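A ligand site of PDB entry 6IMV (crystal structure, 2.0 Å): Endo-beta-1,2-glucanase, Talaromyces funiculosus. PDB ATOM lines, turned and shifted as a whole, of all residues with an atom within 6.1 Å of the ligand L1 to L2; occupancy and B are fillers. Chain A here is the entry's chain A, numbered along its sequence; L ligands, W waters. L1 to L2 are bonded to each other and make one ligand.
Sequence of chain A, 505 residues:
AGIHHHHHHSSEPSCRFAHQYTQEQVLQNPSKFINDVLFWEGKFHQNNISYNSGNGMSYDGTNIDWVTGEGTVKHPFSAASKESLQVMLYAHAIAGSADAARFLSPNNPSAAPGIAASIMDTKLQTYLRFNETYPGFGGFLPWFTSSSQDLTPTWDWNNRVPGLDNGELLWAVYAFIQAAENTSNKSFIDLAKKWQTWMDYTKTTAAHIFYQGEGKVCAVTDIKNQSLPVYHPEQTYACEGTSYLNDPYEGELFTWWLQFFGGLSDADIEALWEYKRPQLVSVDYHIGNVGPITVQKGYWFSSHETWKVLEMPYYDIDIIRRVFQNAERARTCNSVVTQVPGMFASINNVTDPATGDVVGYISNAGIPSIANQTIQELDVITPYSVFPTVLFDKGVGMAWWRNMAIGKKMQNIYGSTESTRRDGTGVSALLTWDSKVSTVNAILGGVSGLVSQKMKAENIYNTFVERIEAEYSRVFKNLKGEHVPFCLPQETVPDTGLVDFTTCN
Residues that only touch the ligand L1 to L2: Pro 162, Tyr 299, Trp 300, Leu 164, Trp 157, Tyr 249, Val 220 and Glu 305. 13 residues have an atom within 4 Å of the ligand L1 to L2: Trp 143, Trp 157, Pro 162, Leu 164, Asp 165, Val 220, Asp 247, Tyr 249, Glu 250, Tyr 299, Trp 300, His 304 and Glu 305. Along chain A the residues within 4 Å of the ligand L1 to L2 span positions 143 to 305.
OE2 of Glu 250 lies within hydrogen-bond range of O3 of LIG L1 (2.5 Å). The side-chain carboxylate (OD1) of Asp 165 is in hydrogen-bond range of an oxygen (O3) of LG2 L2. OD2 of Asp 247 sits at hydrogen-bond distance from O6 of LIG L1 (2.6 Å). A ring nitrogen (NE2) of His 304 sits at hydrogen-bond distance from an oxygen (O4) of LIG L1. The side-chain amino group (NZ) of Lys 82 lies close to an oxygen (O6) of LG3 L3 (3.0 Å). NE1 of Trp 143 sits at hydrogen-bond distance from O3 of LG2 L2 (3.0 Å).
N of Tyr 249 is in hydrogen-bond range of OD1 of Asp 247. N of Trp 300 lies within hydrogen-bond range of OE2 of Glu 305, 2.7 Å away. N of Tyr 299 lies within hydrogen-bond range of OE1 of Glu 305 (2.9 Å). NE2 of His 304 sits close to OE2 of Glu 250. The side-chain carboxylate of Asp 165 is in hydrogen-bond range of the side-chain hydroxyl of Ser 81. The backbone NH (N) of Tyr 299 lies within hydrogen-bond range of the side-chain hydroxyl (OH) of Tyr 249 (3.3 Å).
Water W2 lies within hydrogen-bond range of the side-chain carboxylate of Asp 247, the backbone NH of Gly 251 and an oxygen (O6) of LIG L1.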
ATOM      1  N   ALA A  79     -13.789 -14.829  -5.264  1.00  0.00           N
ATOM      2  CA  ALA A  79     -13.765 -14.368  -3.890  1.00  0.00           C
ATOM      3  C   ALA A  79     -15.010 -14.879  -3.176  1.00  0.00           C
ATOM      4  O   ALA A  79     -15.940 -15.372  -3.825  1.00  0.00           O
ATOM      5  CB  ALA A  79     -13.670 -12.860  -3.846  1.00  0.00           C
ATOM      6  N   SER A  81     -17.399 -13.364  -1.915  1.00  0.00           N
ATOM      7  CA  SER A  81     -18.565 -12.614  -2.375  1.00  0.00           C
ATOM      8  C   SER A  81     -19.288 -13.343  -3.518  1.00  0.00           C
ATOM      9  O   SER A  81     -20.527 -13.441  -3.517  1.00  0.00           O
ATOM     10  CB  SER A  81     -18.152 -11.218  -2.773  1.00  0.00           C
ATOM     11  OG  SER A  81     -16.939 -11.258  -3.521  1.00  0.00           O
ATOM     12  N   LYS A  82     -18.541 -13.886  -4.484  1.00  0.00           N
ATOM     13  CA  LYS A  82     -19.144 -14.658  -5.591  1.00  0.00           C
ATOM     14  C   LYS A  82     -19.580 -16.040  -5.075  1.00  0.00           C
ATOM     15  O   LYS A  82     -20.625 -16.558  -5.445  1.00  0.00           O
ATOM     16  CB  LYS A  82     -18.176 -14.802  -6.770  1.00  0.00           C
ATOM     17  CG  LYS A  82     -17.686 -13.476  -7.349  1.00  0.00           C
ATOM     18  CD  LYS A  82     -16.402 -12.974  -6.748  1.00  0.00           C
ATOM     19  CE  LYS A  82     -16.152 -11.504  -7.017  1.00  0.00           C
ATOM     20  NZ  LYS A  82     -17.236 -10.657  -6.450  1.00  0.00           N
ATOM     21  N   TRP A 143      -9.273 -13.198  -1.859  1.00  0.00           N
ATOM     22  CA  TRP A 143      -9.404 -13.400  -3.313  1.00  0.00           C
ATOM     23  C   TRP A 143      -8.450 -14.525  -3.709  1.00  0.00           C
ATOM     24  O   TRP A 143      -7.307 -14.564  -3.255  1.00  0.00           O
ATOM     25  CB  TRP A 143      -9.108 -12.111  -4.086  1.00  0.00           C
ATOM     26  CG  TRP A 143     -10.198 -11.090  -3.987  1.00  0.00           C
ATOM     27  CD1 TRP A 143     -10.525 -10.332  -2.903  1.00  0.00           C
ATOM     28  CD2 TRP A 143     -11.105 -10.692  -5.033  1.00  0.00           C
ATOM     29  NE1 TRP A 143     -11.564  -9.495  -3.197  1.00  0.00           N
ATOM     30  CE2 TRP A 143     -11.946  -9.703  -4.500  1.00  0.00           C
ATOM     31  CE3 TRP A 143     -11.278 -11.071  -6.367  1.00  0.00           C
ATOM     32  CZ2 TRP A 143     -12.962  -9.104  -5.240  1.00  0.00           C
ATOM     33  CZ3 TRP A 143     -12.275 -10.477  -7.105  1.00  0.00           C
ATOM     34  CH2 TRP A 143     -13.102  -9.503  -6.550  1.00  0.00           C
ATOM     35  N   TRP A 157      -3.401 -10.845  -2.927  1.00  0.00           N
ATOM     36  CA  TRP A 157      -4.141 -11.189  -1.721  1.00  0.00           C
ATOM     37  C   TRP A 157      -3.418 -12.228  -0.868  1.00  0.00           C
ATOM     38  O   TRP A 157      -3.974 -12.692   0.121  1.00  0.00           O
ATOM     39  CB  TRP A 157      -5.569 -11.582  -2.101  1.00  0.00           C
ATOM     40  CG  TRP A 157      -6.386 -10.369  -2.425  1.00  0.00           C
ATOM     41  CD1 TRP A 157      -6.478  -9.746  -3.637  1.00  0.00           C
ATOM     42  CD2 TRP A 157      -7.139  -9.566  -1.505  1.00  0.00           C
ATOM     43  NE1 TRP A 157      -7.270  -8.629  -3.544  1.00  0.00           N
ATOM     44  CE2 TRP A 157      -7.690  -8.492  -2.247  1.00  0.00           C
ATOM     45  CE3 TRP A 157      -7.419  -9.644  -0.137  1.00  0.00           C
ATOM     46  CZ2 TRP A 157      -8.501  -7.523  -1.670  1.00  0.00           C
ATOM     47  CZ3 TRP A 157      -8.234  -8.694   0.431  1.00  0.00           C
ATOM     48  CH2 TRP A 157      -8.757  -7.639  -0.318  1.00  0.00           C
ATOM     49  N   ARG A 160      -3.566 -11.343   3.017  1.00  0.00           N
ATOM     50  CA  ARG A 160      -4.588 -10.289   3.144  1.00  0.00           C
ATOM     51  C   ARG A 160      -5.951 -10.962   3.040  1.00  0.00           C
ATOM     52  O   ARG A 160      -6.119 -11.826   2.169  1.00  0.00           O
ATOM     53  CB  ARG A 160      -4.450  -9.242   2.023  1.00  0.00           C
ATOM     54  CG  ARG A 160      -3.158  -8.444   2.046  1.00  0.00           C
ATOM     55  CD  ARG A 160      -2.990  -7.570   0.811  1.00  0.00           C
ATOM     56  NE  ARG A 160      -3.938  -6.461   0.804  1.00  0.00           N
ATOM     57  CZ  ARG A 160      -4.893  -6.250  -0.102  1.00  0.00           C
ATOM     58  NH1 ARG A 160      -4.957  -6.993  -1.195  1.00  0.00           N
ATOM     59  NH2 ARG A 160      -5.771  -5.287   0.094  1.00  0.00           N
ATOM     60  N   PRO A 162     -10.353 -10.045   3.320  1.00  0.00           N
ATOM     61  CA  PRO A 162     -11.397  -9.037   3.435  1.00  0.00           C
ATOM     62  C   PRO A 162     -12.600  -9.539   4.244  1.00  0.00           C
ATOM     63  O   PRO A 162     -13.114 -10.660   3.980  1.00  0.00           O
ATOM     64  CB  PRO A 162     -11.784  -8.847   1.963  1.00  0.00           C
ATOM     65  CG  PRO A 162     -11.719 -10.246   1.393  1.00  0.00           C
ATOM     66  CD  PRO A 162     -10.593 -10.927   2.158  1.00  0.00           C
ATOM     67  N   LEU A 164     -15.643  -8.120   4.369  1.00  0.00           N
ATOM     68  CA  LEU A 164     -16.922  -7.917   3.694  1.00  0.00           C
ATOM     69  C   LEU A 164     -17.343  -9.190   2.941  1.00  0.00           C
ATOM     70  O   LEU A 164     -18.447  -9.700   3.127  1.00  0.00           O
ATOM     71  CB  LEU A 164     -16.816  -6.719   2.747  1.00  0.00           C
ATOM     72  CG  LEU A 164     -18.123  -6.269   2.085  1.00  0.00           C
ATOM     73  CD1 LEU A 164     -18.136  -4.760   1.914  1.00  0.00           C
ATOM     74  CD2 LEU A 164     -18.319  -6.963   0.734  1.00  0.00           C
ATOM     75  N   ASP A 165     -16.462  -9.666   2.060  1.00  0.00           N
ATOM     76  CA  ASP A 165     -16.769 -10.804   1.197  1.00  0.00           C
ATOM     77  C   ASP A 165     -17.111 -12.029   2.055  1.00  0.00           C
ATOM     78  O   ASP A 165     -17.982 -12.813   1.711  1.00  0.00           O
ATOM     79  CB  ASP A 165     -15.609 -11.127   0.257  1.00  0.00           C
ATOM     80  CG  ASP A 165     -15.138  -9.937  -0.544  1.00  0.00           C
ATOM     81  OD1 ASP A 165     -14.553  -9.039   0.076  1.00  0.00           O
ATOM     82  OD2 ASP A 165     -15.355  -9.923  -1.760  1.00  0.00           O
ATOM     83  N   ALA A 219     -11.589  -3.778   7.495  1.00  0.00           N
ATOM     84  CA  ALA A 219     -12.092  -4.066   6.149  1.00  0.00           C
ATOM     85  C   ALA A 219     -11.194  -5.131   5.503  1.00  0.00           C
ATOM     86  O   ALA A 219     -11.698  -6.104   4.895  1.00  0.00           O
ATOM     87  CB  ALA A 219     -12.141  -2.797   5.333  1.00  0.00           C
ATOM     88  N   VAL A 220      -9.882  -4.953   5.670  1.00  0.00           N
ATOM     89  CA  VAL A 220      -8.892  -5.931   5.226  1.00  0.00           C
ATOM     90  C   VAL A 220      -7.911  -6.164   6.368  1.00  0.00           C
ATOM     91  O   VAL A 220      -7.366  -5.222   6.911  1.00  0.00           O
ATOM     92  CB  VAL A 220      -8.153  -5.471   3.947  1.00  0.00           C
ATOM     93  CG1 VAL A 220      -7.077  -6.464   3.533  1.00  0.00           C
ATOM     94  CG2 VAL A 220      -9.129  -5.219   2.805  1.00  0.00           C
ATOM     95  N   ASP A 247     -20.096   0.835   8.179  1.00  0.00           N
ATOM     96  CA  ASP A 247     -21.198   1.467   7.458  1.00  0.00           C
ATOM     97  C   ASP A 247     -22.362   0.492   7.273  1.00  0.00           C
ATOM     98  O   ASP A 247     -22.255  -0.692   7.570  1.00  0.00           O
ATOM     99  CB  ASP A 247     -20.669   2.068   6.161  1.00  0.00           C
ATOM    100  CG  ASP A 247     -20.165   1.043   5.164  1.00  0.00           C
ATOM    101  OD1 ASP A 247     -20.799  -0.026   5.046  1.00  0.00           O
ATOM    102  OD2 ASP A 247     -19.163   1.339   4.495  1.00  0.00           O
ATOM    103  N   TYR A 249     -23.663  -0.835   4.619  1.00  0.00           N
ATOM    104  CA  TYR A 249     -23.647  -1.567   3.335  1.00  0.00           C
ATOM    105  C   TYR A 249     -23.251  -3.027   3.633  1.00  0.00           C
ATOM    106  O   TYR A 249     -23.565  -3.527   4.692  1.00  0.00           O
ATOM    107  CB  TYR A 249     -22.841  -0.746   2.310  1.00  0.00           C
ATOM    108  CG  TYR A 249     -23.131   0.731   2.438  1.00  0.00           C
ATOM    109  CD1 TYR A 249     -24.417   1.228   2.362  1.00  0.00           C
ATOM    110  CD2 TYR A 249     -22.118   1.632   2.737  1.00  0.00           C
ATOM    111  CE1 TYR A 249     -24.698   2.577   2.554  1.00  0.00           C
ATOM    112  CE2 TYR A 249     -22.370   2.973   2.933  1.00  0.00           C
ATOM    113  CZ  TYR A 249     -23.669   3.453   2.845  1.00  0.00           C
ATOM    114  OH  TYR A 249     -23.902   4.789   3.043  1.00  0.00           O
ATOM    115  N   GLU A 250     -22.595  -3.710   2.678  1.00  0.00           N
ATOM    116  CA  GLU A 250     -22.543  -5.187   2.692  1.00  0.00           C
ATOM    117  C   GLU A 250     -21.724  -5.686   3.880  1.00  0.00           C
ATOM    118  O   GLU A 250     -21.944  -6.795   4.357  1.00  0.00           O
ATOM    119  CB  GLU A 250     -21.940  -5.757   1.406  1.00  0.00           C
ATOM    120  CG  GLU A 250     -22.405  -5.073   0.137  1.00  0.00           C
ATOM    121  CD  GLU A 250     -21.412  -4.041  -0.345  1.00  0.00           C
ATOM    122  OE1 GLU A 250     -21.498  -2.884   0.116  1.00  0.00           O
ATOM    123  OE2 GLU A 250     -20.501  -4.433  -1.123  1.00  0.00           O
ATOM    124  N   GLY A 251     -20.783  -4.851   4.362  1.00  0.00           N
ATOM    125  CA  GLY A 251     -19.931  -5.183   5.481  1.00  0.00           C
ATOM    126  C   GLY A 251     -20.688  -5.400   6.772  1.00  0.00           C
ATOM    127  O   GLY A 251     -20.172  -6.011   7.714  1.00  0.00           O
ATOM    128  N   TYR A 299     -23.069   4.796  -0.190  1.00  0.00           N
ATOM    129  CA  TYR A 299     -21.666   5.080  -0.416  1.00  0.00           C
ATOM    130  C   TYR A 299     -21.562   5.776  -1.777  1.00  0.00           C
ATOM    131  O   TYR A 299     -21.195   6.963  -1.855  1.00  0.00           O
ATOM    132  CB  TYR A 299     -20.809   3.818  -0.267  1.00  0.00           C
ATOM    133  CG  TYR A 299     -19.346   4.111  -0.134  1.00  0.00           C
ATOM    134  CD1 TYR A 299     -18.845   4.777   0.973  1.00  0.00           C
ATOM    135  CD2 TYR A 299     -18.452   3.778  -1.137  1.00  0.00           C
ATOM    136  CE1 TYR A 299     -17.502   5.082   1.102  1.00  0.00           C
ATOM    137  CE2 TYR A 299     -17.103   4.062  -1.027  1.00  0.00           C
ATOM    138  CZ  TYR A 299     -16.629   4.714   0.097  1.00  0.00           C
ATOM    139  OH  TYR A 299     -15.299   4.992   0.184  1.00  0.00           O
ATOM    140  N   TRP A 300     -21.937   5.055  -2.847  1.00  0.00           N
ATOM    141  CA  TRP A 300     -22.245   5.645  -4.156  1.00  0.00           C
ATOM    142  C   TRP A 300     -23.757   5.647  -4.422  1.00  0.00           C
ATOM    143  O   TRP A 300     -24.201   6.300  -5.355  1.00  0.00           O
ATOM    144  CB  TRP A 300     -21.536   4.888  -5.284  1.00  0.00           C
ATOM    145  CG  TRP A 300     -20.049   4.853  -5.141  1.00  0.00           C
ATOM    146  CD1 TRP A 300     -19.186   5.895  -5.317  1.00  0.00           C
ATOM    147  CD2 TRP A 300     -19.246   3.717  -4.790  1.00  0.00           C
ATOM    148  NE1 TRP A 300     -17.910   5.481  -5.072  1.00  0.00           N
ATOM    149  CE2 TRP A 300     -17.908   4.149  -4.765  1.00  0.00           C
ATOM    150  CE3 TRP A 300     -19.536   2.382  -4.488  1.00  0.00           C
ATOM    151  CZ2 TRP A 300     -16.855   3.288  -4.468  1.00  0.00           C
ATOM    152  CZ3 TRP A 300     -18.492   1.532  -4.183  1.00  0.00           C
ATOM    153  CH2 TRP A 300     -17.180   1.983  -4.161  1.00  0.00           C
ATOM    154  N   HIS A 304     -25.455  -2.521  -5.424  1.00  0.00           N
ATOM    155  CA  HIS A 304     -24.747  -3.616  -4.732  1.00  0.00           C
ATOM    156  C   HIS A 304     -24.684  -3.365  -3.217  1.00  0.00           C
ATOM    157  O   HIS A 304     -24.605  -4.320  -2.454  1.00  0.00           O
ATOM    158  CB  HIS A 304     -23.341  -3.866  -5.321  1.00  0.00           C
ATOM    159  CG  HIS A 304     -22.286  -2.991  -4.744  1.00  0.00           C
ATOM    160  ND1 HIS A 304     -22.104  -1.677  -5.140  1.00  0.00           N
ATOM    161  CD2 HIS A 304     -21.355  -3.228  -3.789  1.00  0.00           C
ATOM    162  CE1 HIS A 304     -21.105  -1.141  -4.443  1.00  0.00           C
ATOM    163  NE2 HIS A 304     -20.639  -2.068  -3.623  1.00  0.00           N
ATOM    164  N   GLU A 305     -24.741  -2.091  -2.805  1.00  0.00           N
ATOM    165  CA  GLU A 305     -24.617  -1.700  -1.386  1.00  0.00           C
ATOM    166  C   GLU A 305     -25.760  -2.271  -0.538  1.00  0.00           C
ATOM    167  O   GLU A 305     -25.652  -2.298   0.685  1.00  0.00           O
ATOM    168  CB  GLU A 305     -24.559  -0.173  -1.257  1.00  0.00           C
ATOM    169  CG  GLU A 305     -23.344   0.449  -1.905  1.00  0.00           C
ATOM    170  CD  GLU A 305     -23.451   1.944  -2.188  1.00  0.00           C
ATOM    171  OE1 GLU A 305     -24.298   2.611  -1.559  1.00  0.00           O
ATOM    172  OE2 GLU A 305     -22.705   2.427  -3.063  1.00  0.00           O
HETATM  173  C1  LIG L   1     -15.679  -0.877  -0.387  1.00  0.00           C
HETATM  174  C2  LIG L   1     -16.299  -2.217  -0.700  1.00  0.00           C
HETATM  175  C3  LIG L   1     -17.692  -2.046  -1.287  1.00  0.00           C
HETATM  176  C4  LIG L   1     -18.566  -1.272  -0.310  1.00  0.00           C
HETATM  177  C5  LIG L   1     -17.894   0.064  -0.001  1.00  0.00           C
HETATM  178  C6  LIG L   1     -18.650   0.824   1.091  1.00  0.00           C
HETATM  179  O1  LIG L   1     -15.455  -0.235  -1.661  1.00  0.00           O
HETATM  180  O2  LIG L   1     -15.469  -2.875  -1.664  1.00  0.00           O
HETATM  181  O3  LIG L   1     -18.306  -3.305  -1.560  1.00  0.00           O
HETATM  182  O4  LIG L   1     -19.884  -1.112  -0.858  1.00  0.00           O
HETATM  183  O5  LIG L   1     -16.550  -0.123   0.450  1.00  0.00           O
HETATM  184  O6  LIG L   1     -18.652   0.091   2.314  1.00  0.00           O
HETATM  185  C1  LG2 L   2     -15.323  -5.175  -2.349  1.00  0.00           C
HETATM  186  C2  LG2 L   2     -14.740  -6.531  -1.979  1.00  0.00           C
HETATM  187  C3  LG2 L   2     -13.252  -6.403  -1.658  1.00  0.00           C
HETATM  188  C4  LG2 L   2     -13.094  -5.353  -0.550  1.00  0.00           C
HETATM  189  C5  LG2 L   2     -11.662  -5.076  -0.128  1.00  0.00           C
HETATM  190  C6  LG2 L   2     -15.022  -4.174  -1.252  1.00  0.00           C
HETATM  191  O1  LG2 L   2     -16.732  -5.255  -2.459  1.00  0.00           O
HETATM  192  O2  LG2 L   2     -14.905  -7.466  -3.030  1.00  0.00           O
HETATM  193  O3  LG2 L   2     -12.753  -7.655  -1.221  1.00  0.00           O
HETATM  194  O4  LG2 L   2     -13.639  -4.110  -0.973  1.00  0.00           O
HETATM  195  O5  LG2 L   2     -10.935  -4.626  -1.247  1.00  0.00           O
HETATM  196  C1  LG3 L   3     -12.773  -6.868  -9.924  1.00  0.00           C
HETATM  197  C2  LG3 L   3     -13.270  -7.470 -11.254  1.00  0.00           C
HETATM  198  C3  LG3 L   3     -14.563  -8.291 -11.074  1.00  0.00           C
HETATM  199  C4  LG3 L   3     -15.578  -7.488 -10.236  1.00  0.00           C
HETATM  200  C5  LG3 L   3     -16.872  -8.259  -9.947  1.00  0.00           C
HETATM  201  C6  LG3 L   3     -13.906  -6.166  -9.200  1.00  0.00           C
HETATM  202  O1  LG3 L   3     -13.519  -5.616  -7.933  1.00  0.00           O
HETATM  203  O2  LG3 L   3     -11.756  -5.919 -10.200  1.00  0.00           O
HETATM  204  O3  LG3 L   3     -12.258  -8.287 -11.850  1.00  0.00           O
HETATM  205  O4  LG3 L   3     -15.138  -8.655 -12.347  1.00  0.00           O
HETATM  206  O5  LG3 L   3     -14.976  -7.079  -9.001  1.00  0.00           O
HETATM  207  O6  LG3 L   3     -16.566  -9.391  -9.133  1.00  0.00           O
HETATM  208  O   HOH W   1     -16.625  -1.812   3.213  1.00  0.00           O
HETATM  209  O   HOH W   2     -19.667  -2.177   4.076  1.00  0.00           O
